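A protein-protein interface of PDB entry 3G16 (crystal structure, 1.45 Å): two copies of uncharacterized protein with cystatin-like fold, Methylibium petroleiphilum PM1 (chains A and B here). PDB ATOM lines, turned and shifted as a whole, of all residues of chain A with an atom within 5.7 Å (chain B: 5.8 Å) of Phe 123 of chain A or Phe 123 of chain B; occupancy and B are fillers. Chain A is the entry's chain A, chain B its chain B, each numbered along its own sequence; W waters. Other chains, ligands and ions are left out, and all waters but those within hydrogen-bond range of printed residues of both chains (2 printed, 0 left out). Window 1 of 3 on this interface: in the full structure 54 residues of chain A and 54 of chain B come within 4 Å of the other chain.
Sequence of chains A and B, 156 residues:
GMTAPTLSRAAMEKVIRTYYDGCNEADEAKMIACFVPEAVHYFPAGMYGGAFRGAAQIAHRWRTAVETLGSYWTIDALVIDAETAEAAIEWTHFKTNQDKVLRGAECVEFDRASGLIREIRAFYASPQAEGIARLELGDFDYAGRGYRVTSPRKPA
N of Ala 125 of chain A sits at hydrogen-bond distance from O of Arg 103 of chain A, 2.8 Å away. The backbone NH (N) of Leu 137 of chain A is in hydrogen-bond range of the side-chain hydroxyl (OH) of Tyr 142 of chain A (3.0 Å). The backbone carbonyl oxygen (O) of Arg 103 of chain B lies within hydrogen-bond range of the backbone NH (N) of Ala 125 of chain B, at 2.8 Å. The backbone carbonyl oxygen (O) of Ala 105 of chain B lies within hydrogen-bond range of the backbone NH (N) of Phe 123 of chain B, at 2.8 Å. The backbone carbonyl oxygen (O) of Arg 121 of chain B sits at hydrogen-bond distance from the backbone NH (N) of Cys 107 of chain B (2.8 Å). N of Leu 137 of chain B is in hydrogen-bond range of OH of Tyr 142 of chain B (2.9 Å).
Of chain B, only Glu 90 (3.4 Å), Gly 104 (3.5 Å), Ala 105 (3.6 Å), Phe 123 (3.9 Å), Tyr 124 (3.6 Å) and Ala 125 (3.8 Å) come within 4 Å of Phe 123 of chain A. Phe 123 of chain B touches six residues of chain A. Of the printed residues of chain A, Gly 104 of chain B touches Phe 123. Of the printed residues of chain B, Glu 90 of chain A touches Arg 121 and Phe 123. The nearest residue of chain B that does not touch Phe 123 of chain A is Arg 103 of chain B (4.6 Å).
The side-chain carboxylate of Glu 90 of chain A is in salt-bridge range of the guanidinium group of Arg 121 of chain B. The guanidinium group (NE) of Arg 121 of chain A is in salt-bridge range of the side-chain carboxylate (OE2) of Glu 90 of chain B, at 2.8 Å. N of Tyr 124 of chain A sits at hydrogen-bond distance from O of Tyr 124 of chain B (2.8 Å).
Glu 90 of chain A touches Phe 123 of chain B, and with the chains exchanged Phe 123 of chain A touches Glu 90 of chain B. Arg 103 of chain A touches Tyr 142 of chain B, and with the chains exchanged Tyr 142 of chain A touches Arg 103 of chain B. Phe 123 of chain A touches Tyr 124 of chain B, and with the chains exchanged Tyr 124 of chain A touches Phe 123 of chain B. Phe 123 of chain A touches Ala 125 of chain B, and with the chains exchanged Ala 125 of chain A touches Phe 123 of chain B. 15 positions are printed for both chains.
Water W2 lies within hydrogen-bond range of the side-chain hydroxyl of Tyr 142 of chain A (2.7 Å) and the side-chain carboxylate of Glu 90 of chain B (2.8 Å). Water W1 lies within hydrogen-bond range of OH of Tyr 142 of chain B (2.7 Å) and OE2 of Glu 90 of chain A (2.8 Å).
Among the printed residues, merely in contact across the chains: Tyr 142 of chain A with Arg 103 of chain B (3.3 Å), Phe 123 of chain A with Glu 90 of chain B (3.4 Å), Glu 90 of chain A with Phe 123 of chain B (3.4 Å), Arg 103 of chain A with Tyr 142 of chain B (3.4 Å), Phe 123 of chain A with Gly 104 of chain B (3.5 Å), Ala 105 of chain A with Phe 123 of chain B (3.6 Å), Phe 123 of chain A with Ala 105 of chain B (3.6 Å), Tyr 124 of chain A with Phe 123 of chain B (3.6 Å), Phe 123 of chain A with Tyr 124 of chain B (3.6 Å), Gly 104 of chain A with Phe 123 of chain B (3.6 Å), Pro 44 of chain A with Ala 125 of chain B (3.6 Å), Ala 125 of chain A with Pro 44 of chain B (3.6 Å), Ala 125 of chain A with Phe 123 of chain B (3.7 Å), Phe 123 of chain A with Ala 125 of chain B (3.8 Å), Phe 123 of chain A with Phe 123 of chain B (3.9 Å) and Ala 125 of chain A with Leu 137 of chain B (3.9 Å).
Hydrophobic or aromatic side chains of chain B within 4 Å of the printed part of chain A: Pro 44, Ala 105, Phe 123, Ala 125 and Tyr 142. Of the 15 printed residues of chain A, 10 touch a printed residue of chain B. Hydrophobic or aromatic side chains of chain A within 4 Å of the printed part of chain B: Pro 44, Ala 105, Phe 123, Ala 125 and Tyr 142. Along chain A the printed residues that touch a printed residue of chain B span positions 44 to 142. Among the printed residues, 19 pairs touch across the chains. Among the printed residues, Asp or Glu carboxylates within 4 Å of a Lys or Arg side-chain nitrogen of the other chain: Glu 90 of chain A with Arg 121 of chain B and Arg 121 of chain A with Glu 90 of chain B.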
ATOM      1  N   PRO A  44      36.073   9.854  -2.572  1.00  0.00           N
ATOM      2  CA  PRO A  44      36.805   8.600  -2.751  1.00  0.00           C
ATOM      3  C   PRO A  44      38.241   8.695  -2.254  1.00  0.00           C
ATOM      4  O   PRO A  44      38.897   9.745  -2.454  1.00  0.00           O
ATOM      5  CB  PRO A  44      36.724   8.394  -4.265  1.00  0.00           C
ATOM      6  CG  PRO A  44      35.494   9.052  -4.674  1.00  0.00           C
ATOM      7  CD  PRO A  44      35.380  10.284  -3.789  1.00  0.00           C
ATOM      8  N   GLU A  90      22.470  13.844  -7.059  1.00  0.00           N
ATOM      9  CA  GLU A  90      23.221  13.422  -8.250  1.00  0.00           C
ATOM     10  C   GLU A  90      23.668  14.726  -8.864  1.00  0.00           C
ATOM     11  O   GLU A  90      22.847  15.637  -9.011  1.00  0.00           O
ATOM     12  CB  GLU A  90      22.375  12.645  -9.244  1.00  0.00           C
ATOM     13  CG  GLU A  90      23.124  12.034 -10.396  1.00  0.00           C
ATOM     14  CD  GLU A  90      22.197  11.388 -11.407  1.00  0.00           C
ATOM     15  OE1 GLU A  90      21.036  11.871 -11.540  1.00  0.00           O
ATOM     16  OE2 GLU A  90      22.616  10.425 -12.064  1.00  0.00           O
ATOM     17  N   TRP A  91      24.963  14.850  -9.127  1.00  0.00           N
ATOM     18  CA  TRP A  91      25.534  16.112  -9.530  1.00  0.00           C
ATOM     19  C   TRP A  91      26.503  15.986 -10.706  1.00  0.00           C
ATOM     20  O   TRP A  91      26.960  14.877 -11.046  1.00  0.00           O
ATOM     21  CB  TRP A  91      26.248  16.768  -8.314  1.00  0.00           C
ATOM     22  CG  TRP A  91      27.247  15.858  -7.646  1.00  0.00           C
ATOM     23  CD1 TRP A  91      27.035  15.187  -6.481  1.00  0.00           C
ATOM     24  CD2 TRP A  91      28.571  15.482  -8.080  1.00  0.00           C
ATOM     25  NE1 TRP A  91      28.122  14.395  -6.171  1.00  0.00           N
ATOM     26  CE2 TRP A  91      29.092  14.577  -7.115  1.00  0.00           C
ATOM     27  CE3 TRP A  91      29.384  15.855  -9.149  1.00  0.00           C
ATOM     28  CZ2 TRP A  91      30.367  14.008  -7.227  1.00  0.00           C
ATOM     29  CZ3 TRP A  91      30.654  15.293  -9.261  1.00  0.00           C
ATOM     30  CH2 TRP A  91      31.126  14.375  -8.296  1.00  0.00           C
ATOM     31  N   ARG A 103      30.791  13.367 -13.214  1.00  0.00           N
ATOM     32  CA  ARG A 103      29.486  13.226 -12.591  1.00  0.00           C
ATOM     33  C   ARG A 103      29.597  12.298 -11.388  1.00  0.00           C
ATOM     34  O   ARG A 103      30.492  11.482 -11.280  1.00  0.00           O
ATOM     35  CB  ARG A 103      28.489  12.707 -13.589  1.00  0.00           C
ATOM     36  CG  ARG A 103      28.426  13.607 -14.827  1.00  0.00           C
ATOM     37  CD  ARG A 103      27.189  13.342 -15.591  1.00  0.00           C
ATOM     38  NE  ARG A 103      27.173  13.800 -16.996  1.00  0.00           N
ATOM     39  CZ  ARG A 103      26.487  14.832 -17.476  1.00  0.00           C
ATOM     40  NH1 ARG A 103      25.805  15.642 -16.698  1.00  0.00           N
ATOM     41  NH2 ARG A 103      26.459  15.038 -18.781  1.00  0.00           N
ATOM     42  N   GLY A 104      28.673  12.434 -10.475  1.00  0.00           N
ATOM     43  CA  GLY A 104      28.655  11.630  -9.268  1.00  0.00           C
ATOM     44  C   GLY A 104      27.402  11.771  -8.466  1.00  0.00           C
ATOM     45  O   GLY A 104      26.431  12.390  -8.910  1.00  0.00           O
ATOM     46  N   ALA A 105      27.435  11.242  -7.251  1.00  0.00           N
ATOM     47  CA  ALA A 105      26.308  11.376  -6.335  1.00  0.00           C
ATOM     48  C   ALA A 105      26.872  11.488  -4.943  1.00  0.00           C
ATOM     49  O   ALA A 105      27.998  11.048  -4.681  1.00  0.00           O
ATOM     50  CB  ALA A 105      25.347  10.210  -6.462  1.00  0.00           C
ATOM     51  N   GLU A 106      26.111  12.129  -4.065  1.00  0.00           N
ATOM     52  CA  GLU A 106      26.575  12.263  -2.690  1.00  0.00           C
ATOM     53  C   GLU A 106      25.453  12.158  -1.696  1.00  0.00           C
ATOM     54  O   GLU A 106      24.313  12.517  -1.985  1.00  0.00           O
ATOM     55  CB  GLU A 106      27.338  13.544  -2.491  1.00  0.00           C
ATOM     56  CG  GLU A 106      26.523  14.837  -2.692  1.00  0.00           C
ATOM     57  CD  GLU A 106      27.425  16.065  -2.893  1.00  0.00           C
ATOM     58  OE1 GLU A 106      28.595  15.912  -3.212  1.00  0.00           O
ATOM     59  OE2 GLU A 106      26.884  17.193  -2.785  1.00  0.00           O
ATOM     60  N   CYS A 107      25.792  11.620  -0.517  1.00  0.00           N
ATOM     61  CA  CYS A 107      24.868  11.559   0.616  1.00  0.00           C
ATOM     62  C   CYS A 107      25.124  12.755   1.484  1.00  0.00           C
ATOM     63  O   CYS A 107      26.300  13.104   1.738  1.00  0.00           O
ATOM     64  CB  CYS A 107      25.109  10.309   1.415  1.00  0.00           C
ATOM     65  SG  CYS A 107      24.678   8.790   0.476  1.00  0.00           S
ATOM     66  N   ARG A 121      29.161  12.853   1.804  1.00  0.00           N
ATOM     67  CA  ARG A 121      29.978  11.703   1.354  1.00  0.00           C
ATOM     68  C   ARG A 121      29.756  11.590  -0.141  1.00  0.00           C
ATOM     69  O   ARG A 121      28.649  11.265  -0.561  1.00  0.00           O
ATOM     70  CB  ARG A 121      29.557  10.444   2.092  1.00  0.00           C
ATOM     71  CG  ARG A 121      29.697  10.540   3.608  1.00  0.00           C
ATOM     72  CD  ARG A 121      29.495   9.212   4.300  1.00  0.00           C
ATOM     73  NE  ARG A 121      28.212   8.578   4.075  1.00  0.00           N
ATOM     74  CZ  ARG A 121      27.091   8.908   4.716  1.00  0.00           C
ATOM     75  NH1 ARG A 121      27.058   9.886   5.605  1.00  0.00           N
ATOM     76  NH2 ARG A 121      25.980   8.230   4.479  1.00  0.00           N
ATOM     77  N   ALA A 122      30.823  11.816  -0.932  1.00  0.00           N
ATOM     78  CA  ALA A 122      30.685  11.835  -2.393  1.00  0.00           C
ATOM     79  C   ALA A 122      31.317  10.635  -3.085  1.00  0.00           C
ATOM     80  O   ALA A 122      32.357  10.114  -2.665  1.00  0.00           O
ATOM     81  CB  ALA A 122      31.309  13.105  -2.977  1.00  0.00           C
ATOM     82  N   PHE A 123      30.642  10.226  -4.153  1.00  0.00           N
ATOM     83  CA  PHE A 123      30.965   9.047  -4.970  1.00  0.00           C
ATOM     84  C   PHE A 123      30.969   9.491  -6.415  1.00  0.00           C
ATOM     85  O   PHE A 123      30.254  10.439  -6.772  1.00  0.00           O
ATOM     86  CB  PHE A 123      29.931   7.958  -4.758  1.00  0.00           C
ATOM     87  CG  PHE A 123      29.785   7.590  -3.304  1.00  0.00           C
ATOM     88  CD1 PHE A 123      30.578   6.637  -2.721  1.00  0.00           C
ATOM     89  CD2 PHE A 123      28.907   8.275  -2.492  1.00  0.00           C
ATOM     90  CE1 PHE A 123      30.482   6.322  -1.359  1.00  0.00           C
ATOM     91  CE2 PHE A 123      28.793   7.979  -1.127  1.00  0.00           C
ATOM     92  CZ  PHE A 123      29.575   7.002  -0.584  1.00  0.00           C
ATOM     93  N   TYR A 124      31.721   8.793  -7.252  1.00  0.00           N
ATOM     94  CA  TYR A 124      31.926   9.210  -8.630  1.00  0.00           C
ATOM     95  C   TYR A 124      31.491   8.231  -9.673  1.00  0.00           C
ATOM     96  O   TYR A 124      31.586   7.016  -9.477  1.00  0.00           O
ATOM     97  CB  TYR A 124      33.415   9.445  -8.890  1.00  0.00           C
ATOM     98  CG  TYR A 124      34.106  10.549  -8.134  1.00  0.00           C
ATOM     99  CD1 TYR A 124      33.403  11.576  -7.489  1.00  0.00           C
ATOM    100  CD2 TYR A 124      35.500  10.621  -8.146  1.00  0.00           C
ATOM    101  CE1 TYR A 124      34.103  12.640  -6.846  1.00  0.00           C
ATOM    102  CE2 TYR A 124      36.174  11.660  -7.517  1.00  0.00           C
ATOM    103  CZ  TYR A 124      35.469  12.635  -6.872  1.00  0.00           C
ATOM    104  OH  TYR A 124      36.122  13.686  -6.282  1.00  0.00           O
ATOM    105  N   ALA A 125      31.109   8.759 -10.848  1.00  0.00           N
ATOM    106  CA  ALA A 125      30.896   7.925 -12.023  1.00  0.00           C
ATOM    107  C   ALA A 125      32.250   7.663 -12.668  1.00  0.00           C
ATOM    108  O   ALA A 125      32.496   8.032 -13.828  1.00  0.00           O
ATOM    109  CB  ALA A 125      29.965   8.640 -13.020  1.00  0.00           C
ATOM    110  N   LEU A 137      35.716   5.646   1.022  1.00  0.00           N
ATOM    111  CA  LEU A 137      35.965   7.060   1.260  1.00  0.00           C
ATOM    112  C   LEU A 137      37.214   7.259   2.075  1.00  0.00           C
ATOM    113  O   LEU A 137      37.464   6.570   3.049  1.00  0.00           O
ATOM    114  CB  LEU A 137      34.800   7.648   1.996  1.00  0.00           C
ATOM    115  CG  LEU A 137      33.449   7.634   1.298  1.00  0.00           C
ATOM    116  CD1 LEU A 137      32.340   7.947   2.312  1.00  0.00           C
ATOM    117  CD2 LEU A 137      33.427   8.565   0.032  1.00  0.00           C
ATOM    118  N   TYR A 142      34.944   4.096   9.062  1.00  0.00           N
ATOM    119  CA  TYR A 142      33.953   3.043   8.874  1.00  0.00           C
ATOM    120  C   TYR A 142      33.697   2.201  10.126  1.00  0.00           C
ATOM    121  O   TYR A 142      32.574   1.933  10.460  1.00  0.00           O
ATOM    122  CB  TYR A 142      34.359   2.129   7.704  1.00  0.00           C
ATOM    123  CG  TYR A 142      34.170   2.778   6.347  1.00  0.00           C
ATOM    124  CD1 TYR A 142      32.901   2.871   5.804  1.00  0.00           C
ATOM    125  CD2 TYR A 142      35.216   3.369   5.641  1.00  0.00           C
ATOM    126  CE1 TYR A 142      32.669   3.503   4.588  1.00  0.00           C
ATOM    127  CE2 TYR A 142      34.979   3.995   4.415  1.00  0.00           C
ATOM    128  CZ  TYR A 142      33.703   4.067   3.913  1.00  0.00           C
ATOM    129  OH  TYR A 142      33.485   4.676   2.698  1.00  0.00           O
ATOM    130  N   PRO B  44      29.228   3.374 -13.792  1.00  0.00           N
ATOM    131  CA  PRO B  44      30.234   4.238 -14.398  1.00  0.00           C
ATOM    132  C   PRO B  44      30.722   3.705 -15.734  1.00  0.00           C
ATOM    133  O   PRO B  44      30.874   2.494 -15.887  1.00  0.00           O
ATOM    134  CB  PRO B  44      31.348   4.233 -13.345  1.00  0.00           C
ATOM    135  CG  PRO B  44      30.603   4.081 -12.039  1.00  0.00           C
ATOM    136  CD  PRO B  44      29.584   3.037 -12.409  1.00  0.00           C
ATOM    137  N   GLU B  90      23.531   4.055  -0.013  1.00  0.00           N
ATOM    138  CA  GLU B  90      24.996   3.971   0.167  1.00  0.00           C
ATOM    139  C   GLU B  90      25.229   2.491   0.484  1.00  0.00           C
ATOM    140  O   GLU B  90      24.549   1.948   1.357  1.00  0.00           O
ATOM    141  CB  GLU B  90      25.491   4.836   1.306  1.00  0.00           C
ATOM    142  CG  GLU B  90      26.992   4.885   1.409  1.00  0.00           C
ATOM    143  CD  GLU B  90      27.488   5.628   2.620  1.00  0.00           C
ATOM    144  OE1 GLU B  90      26.789   5.565   3.675  1.00  0.00           O
ATOM    145  OE2 GLU B  90      28.589   6.196   2.566  1.00  0.00           O
ATOM    146  N   TRP B  91      26.108   1.845  -0.280  1.00  0.00           N
ATOM    147  CA  TRP B  91      26.263   0.395  -0.198  1.00  0.00           C
ATOM    148  C   TRP B  91      27.745   0.001  -0.185  1.00  0.00           C
ATOM    149  O   TRP B  91      28.668   0.751  -0.545  1.00  0.00           O
ATOM    150  CB  TRP B  91      25.570  -0.307  -1.406  1.00  0.00           C
ATOM    151  CG  TRP B  91      25.928   0.290  -2.749  1.00  0.00           C
ATOM    152  CD1 TRP B  91      25.168   1.180  -3.452  1.00  0.00           C
ATOM    153  CD2 TRP B  91      27.108   0.052  -3.528  1.00  0.00           C
ATOM    154  NE1 TRP B  91      25.828   1.532  -4.585  1.00  0.00           N
ATOM    155  CE2 TRP B  91      27.003   0.825  -4.685  1.00  0.00           C
ATOM    156  CE3 TRP B  91      28.226  -0.763  -3.370  1.00  0.00           C
ATOM    157  CZ2 TRP B  91      27.999   0.858  -5.648  1.00  0.00           C
ATOM    158  CZ3 TRP B  91      29.219  -0.726  -4.307  1.00  0.00           C
ATOM    159  CH2 TRP B  91      29.084   0.072  -5.460  1.00  0.00           C
ATOM    160  N   ARG B 103      32.957   0.328  -2.260  1.00  0.00           N
ATOM    161  CA  ARG B 103      31.826   1.037  -1.696  1.00  0.00           C
ATOM    162  C   ARG B 103      31.335   2.015  -2.727  1.00  0.00           C
ATOM    163  O   ARG B 103      32.048   2.416  -3.619  1.00  0.00           O
ATOM    164  CB  ARG B 103      32.196   1.726  -0.410  1.00  0.00           C
ATOM    165  CG  ARG B 103      32.798   0.774   0.612  1.00  0.00           C
ATOM    166  CD  ARG B 103      32.772   1.365   2.023  1.00  0.00           C
ATOM    167  NE  ARG B 103      33.626   0.710   3.011  1.00  0.00           N
ATOM    168  CZ  ARG B 103      33.226  -0.046   4.025  1.00  0.00           C
ATOM    169  NH1 ARG B 103      31.953  -0.397   4.165  1.00  0.00           N
ATOM    170  NH2 ARG B 103      34.113  -0.461   4.906  1.00  0.00           N
ATOM    171  N   GLY B 104      30.084   2.430  -2.591  1.00  0.00           N
ATOM    172  CA  GLY B 104      29.506   3.365  -3.540  1.00  0.00           C
ATOM    173  C   GLY B 104      28.119   3.777  -3.135  1.00  0.00           C
ATOM    174  O   GLY B 104      27.675   3.570  -2.001  1.00  0.00           O
ATOM    175  N   ALA B 105      27.430   4.451  -4.024  1.00  0.00           N
ATOM    176  CA  ALA B 105      26.064   4.871  -3.758  1.00  0.00           C
ATOM    177  C   ALA B 105      25.295   4.772  -5.065  1.00  0.00           C
ATOM    178  O   ALA B 105      25.888   4.817  -6.171  1.00  0.00           O
ATOM    179  CB  ALA B 105      26.032   6.306  -3.198  1.00  0.00           C
ATOM    180  N   GLU B 106      23.985   4.619  -4.968  1.00  0.00           N
ATOM    181  CA  GLU B 106      23.184   4.581  -6.182  1.00  0.00           C
ATOM    182  C   GLU B 106      21.865   5.276  -6.004  1.00  0.00           C
ATOM    183  O   GLU B 106      21.294   5.275  -4.903  1.00  0.00           O
ATOM    184  CB  GLU B 106      22.955   3.167  -6.674  1.00  0.00           C
ATOM    185  CG  GLU B 106      22.251   2.196  -5.722  1.00  0.00           C
ATOM    186  CD  GLU B 106      22.478   0.734  -6.066  1.00  0.00           C
ATOM    187  OE1 GLU B 106      23.407   0.434  -6.803  1.00  0.00           O
ATOM    188  OE2 GLU B 106      21.698  -0.093  -5.549  1.00  0.00           O
ATOM    189  N   CYS B 107      21.409   5.911  -7.093  1.00  0.00           N
ATOM    190  CA  CYS B 107      20.105   6.511  -7.144  1.00  0.00           C
ATOM    191  C   CYS B 107      19.116   5.488  -7.704  1.00  0.00           C
ATOM    192  O   CYS B 107      19.432   4.770  -8.656  1.00  0.00           O
ATOM    193  CB  CYS B 107      20.122   7.737  -8.012  1.00  0.00           C
ATOM    194  SG  CYS B 107      21.168   9.063  -7.427  1.00  0.00           S
ATOM    195  N   ARG B 121      21.049   3.919 -10.856  1.00  0.00           N
ATOM    196  CA  ARG B 121      22.250   4.587 -11.387  1.00  0.00           C
ATOM    197  C   ARG B 121      23.299   4.521 -10.270  1.00  0.00           C
ATOM    198  O   ARG B 121      23.110   5.142  -9.210  1.00  0.00           O
ATOM    199  CB  ARG B 121      21.969   6.043 -11.789  1.00  0.00           C
ATOM    200  CG  ARG B 121      20.886   6.164 -12.830  1.00  0.00           C
ATOM    201  CD  ARG B 121      20.724   7.585 -13.329  1.00  0.00           C
ATOM    202  NE  ARG B 121      20.410   8.596 -12.310  1.00  0.00           N
ATOM    203  CZ  ARG B 121      19.195   8.894 -11.871  1.00  0.00           C
ATOM    204  NH1 ARG B 121      18.147   8.142 -12.198  1.00  0.00           N
ATOM    205  NH2 ARG B 121      19.026   9.868 -10.987  1.00  0.00           N
ATOM    206  N   ALA B 122      24.375   3.761 -10.486  1.00  0.00           N
ATOM    207  CA  ALA B 122      25.402   3.532  -9.473  1.00  0.00           C
ATOM    208  C   ALA B 122      26.693   4.330  -9.732  1.00  0.00           C
ATOM    209  O   ALA B 122      27.154   4.523 -10.876  1.00  0.00           O
ATOM    210  CB  ALA B 122      25.739   2.019  -9.372  1.00  0.00           C
ATOM    211  N   PHE B 123      27.282   4.710  -8.579  1.00  0.00           N
ATOM    212  CA  PHE B 123      28.502   5.521  -8.473  1.00  0.00           C
ATOM    213  C   PHE B 123      29.433   4.854  -7.461  1.00  0.00           C
ATOM    214  O   PHE B 123      28.956   4.158  -6.555  1.00  0.00           O
ATOM    215  CB  PHE B 123      28.154   6.955  -8.035  1.00  0.00           C
ATOM    216  CG  PHE B 123      27.130   7.600  -8.934  1.00  0.00           C
ATOM    217  CD1 PHE B 123      27.492   8.330 -10.042  1.00  0.00           C
ATOM    218  CD2 PHE B 123      25.800   7.458  -8.659  1.00  0.00           C
ATOM    219  CE1 PHE B 123      26.520   8.896 -10.875  1.00  0.00           C
ATOM    220  CE2 PHE B 123      24.839   8.005  -9.472  1.00  0.00           C
ATOM    221  CZ  PHE B 123      25.202   8.749 -10.582  1.00  0.00           C
ATOM    222  N   TYR B 124      30.732   5.059  -7.605  1.00  0.00           N
ATOM    223  CA  TYR B 124      31.719   4.334  -6.794  1.00  0.00           C
ATOM    224  C   TYR B 124      32.602   5.247  -5.982  1.00  0.00           C
ATOM    225  O   TYR B 124      32.915   6.382  -6.361  1.00  0.00           O
ATOM    226  CB  TYR B 124      32.658   3.563  -7.701  1.00  0.00           C
ATOM    227  CG  TYR B 124      32.034   2.515  -8.570  1.00  0.00           C
ATOM    228  CD1 TYR B 124      30.816   1.910  -8.251  1.00  0.00           C
ATOM    229  CD2 TYR B 124      32.697   2.069  -9.706  1.00  0.00           C
ATOM    230  CE1 TYR B 124      30.282   0.897  -9.079  1.00  0.00           C
ATOM    231  CE2 TYR B 124      32.147   1.059 -10.503  1.00  0.00           C
ATOM    232  CZ  TYR B 124      30.968   0.476 -10.161  1.00  0.00           C
ATOM    233  OH  TYR B 124      30.415  -0.523 -10.967  1.00  0.00           O
ATOM    234  N   ALA B 125      33.066   4.716  -4.864  1.00  0.00           N
ATOM    235  CA  ALA B 125      34.124   5.375  -4.081  1.00  0.00           C
ATOM    236  C   ALA B 125      35.474   5.052  -4.716  1.00  0.00           C
ATOM    237  O   ALA B 125      36.332   4.432  -4.114  1.00  0.00           O
ATOM    238  CB  ALA B 125      34.091   4.927  -2.571  1.00  0.00           C
ATOM    239  N   LEU B 137      27.967   8.059 -16.354  1.00  0.00           N
ATOM    240  CA  LEU B 137      27.411   6.713 -16.487  1.00  0.00           C
ATOM    241  C   LEU B 137      27.464   6.207 -17.934  1.00  0.00           C
ATOM    242  O   LEU B 137      27.194   6.942 -18.871  1.00  0.00           O
ATOM    243  CB  LEU B 137      25.969   6.701 -16.021  1.00  0.00           C
ATOM    244  CG  LEU B 137      25.723   7.099 -14.571  1.00  0.00           C
ATOM    245  CD1 LEU B 137      24.257   7.408 -14.380  1.00  0.00           C
ATOM    246  CD2 LEU B 137      26.219   6.017 -13.649  1.00  0.00           C
ATOM    247  N   TYR B 142      22.198  11.147 -21.360  1.00  0.00           N
ATOM    248  CA  TYR B 142      22.184  12.404 -20.631  1.00  0.00           C
ATOM    249  C   TYR B 142      21.429  13.514 -21.373  1.00  0.00           C
ATOM    250  O   TYR B 142      20.598  14.207 -20.772  1.00  0.00           O
ATOM    251  CB  TYR B 142      23.608  12.860 -20.341  1.00  0.00           C
ATOM    252  CG  TYR B 142      24.260  12.088 -19.202  1.00  0.00           C
ATOM    253  CD1 TYR B 142      23.899  12.385 -17.897  1.00  0.00           C
ATOM    254  CD2 TYR B 142      25.148  11.034 -19.435  1.00  0.00           C
ATOM    255  CE1 TYR B 142      24.446  11.705 -16.821  1.00  0.00           C
ATOM    256  CE2 TYR B 142      25.731  10.355 -18.343  1.00  0.00           C
ATOM    257  CZ  TYR B 142      25.346  10.676 -17.061  1.00  0.00           C
ATOM    258  OH  TYR B 142      25.878  10.040 -15.954  1.00  0.00           O
HETATM  259  O   HOH W   1      24.911  10.884 -13.617  1.00  0.00           O
HETATM  260  O   HOH W   2      30.928   4.738   2.004  1.00  0.00           O
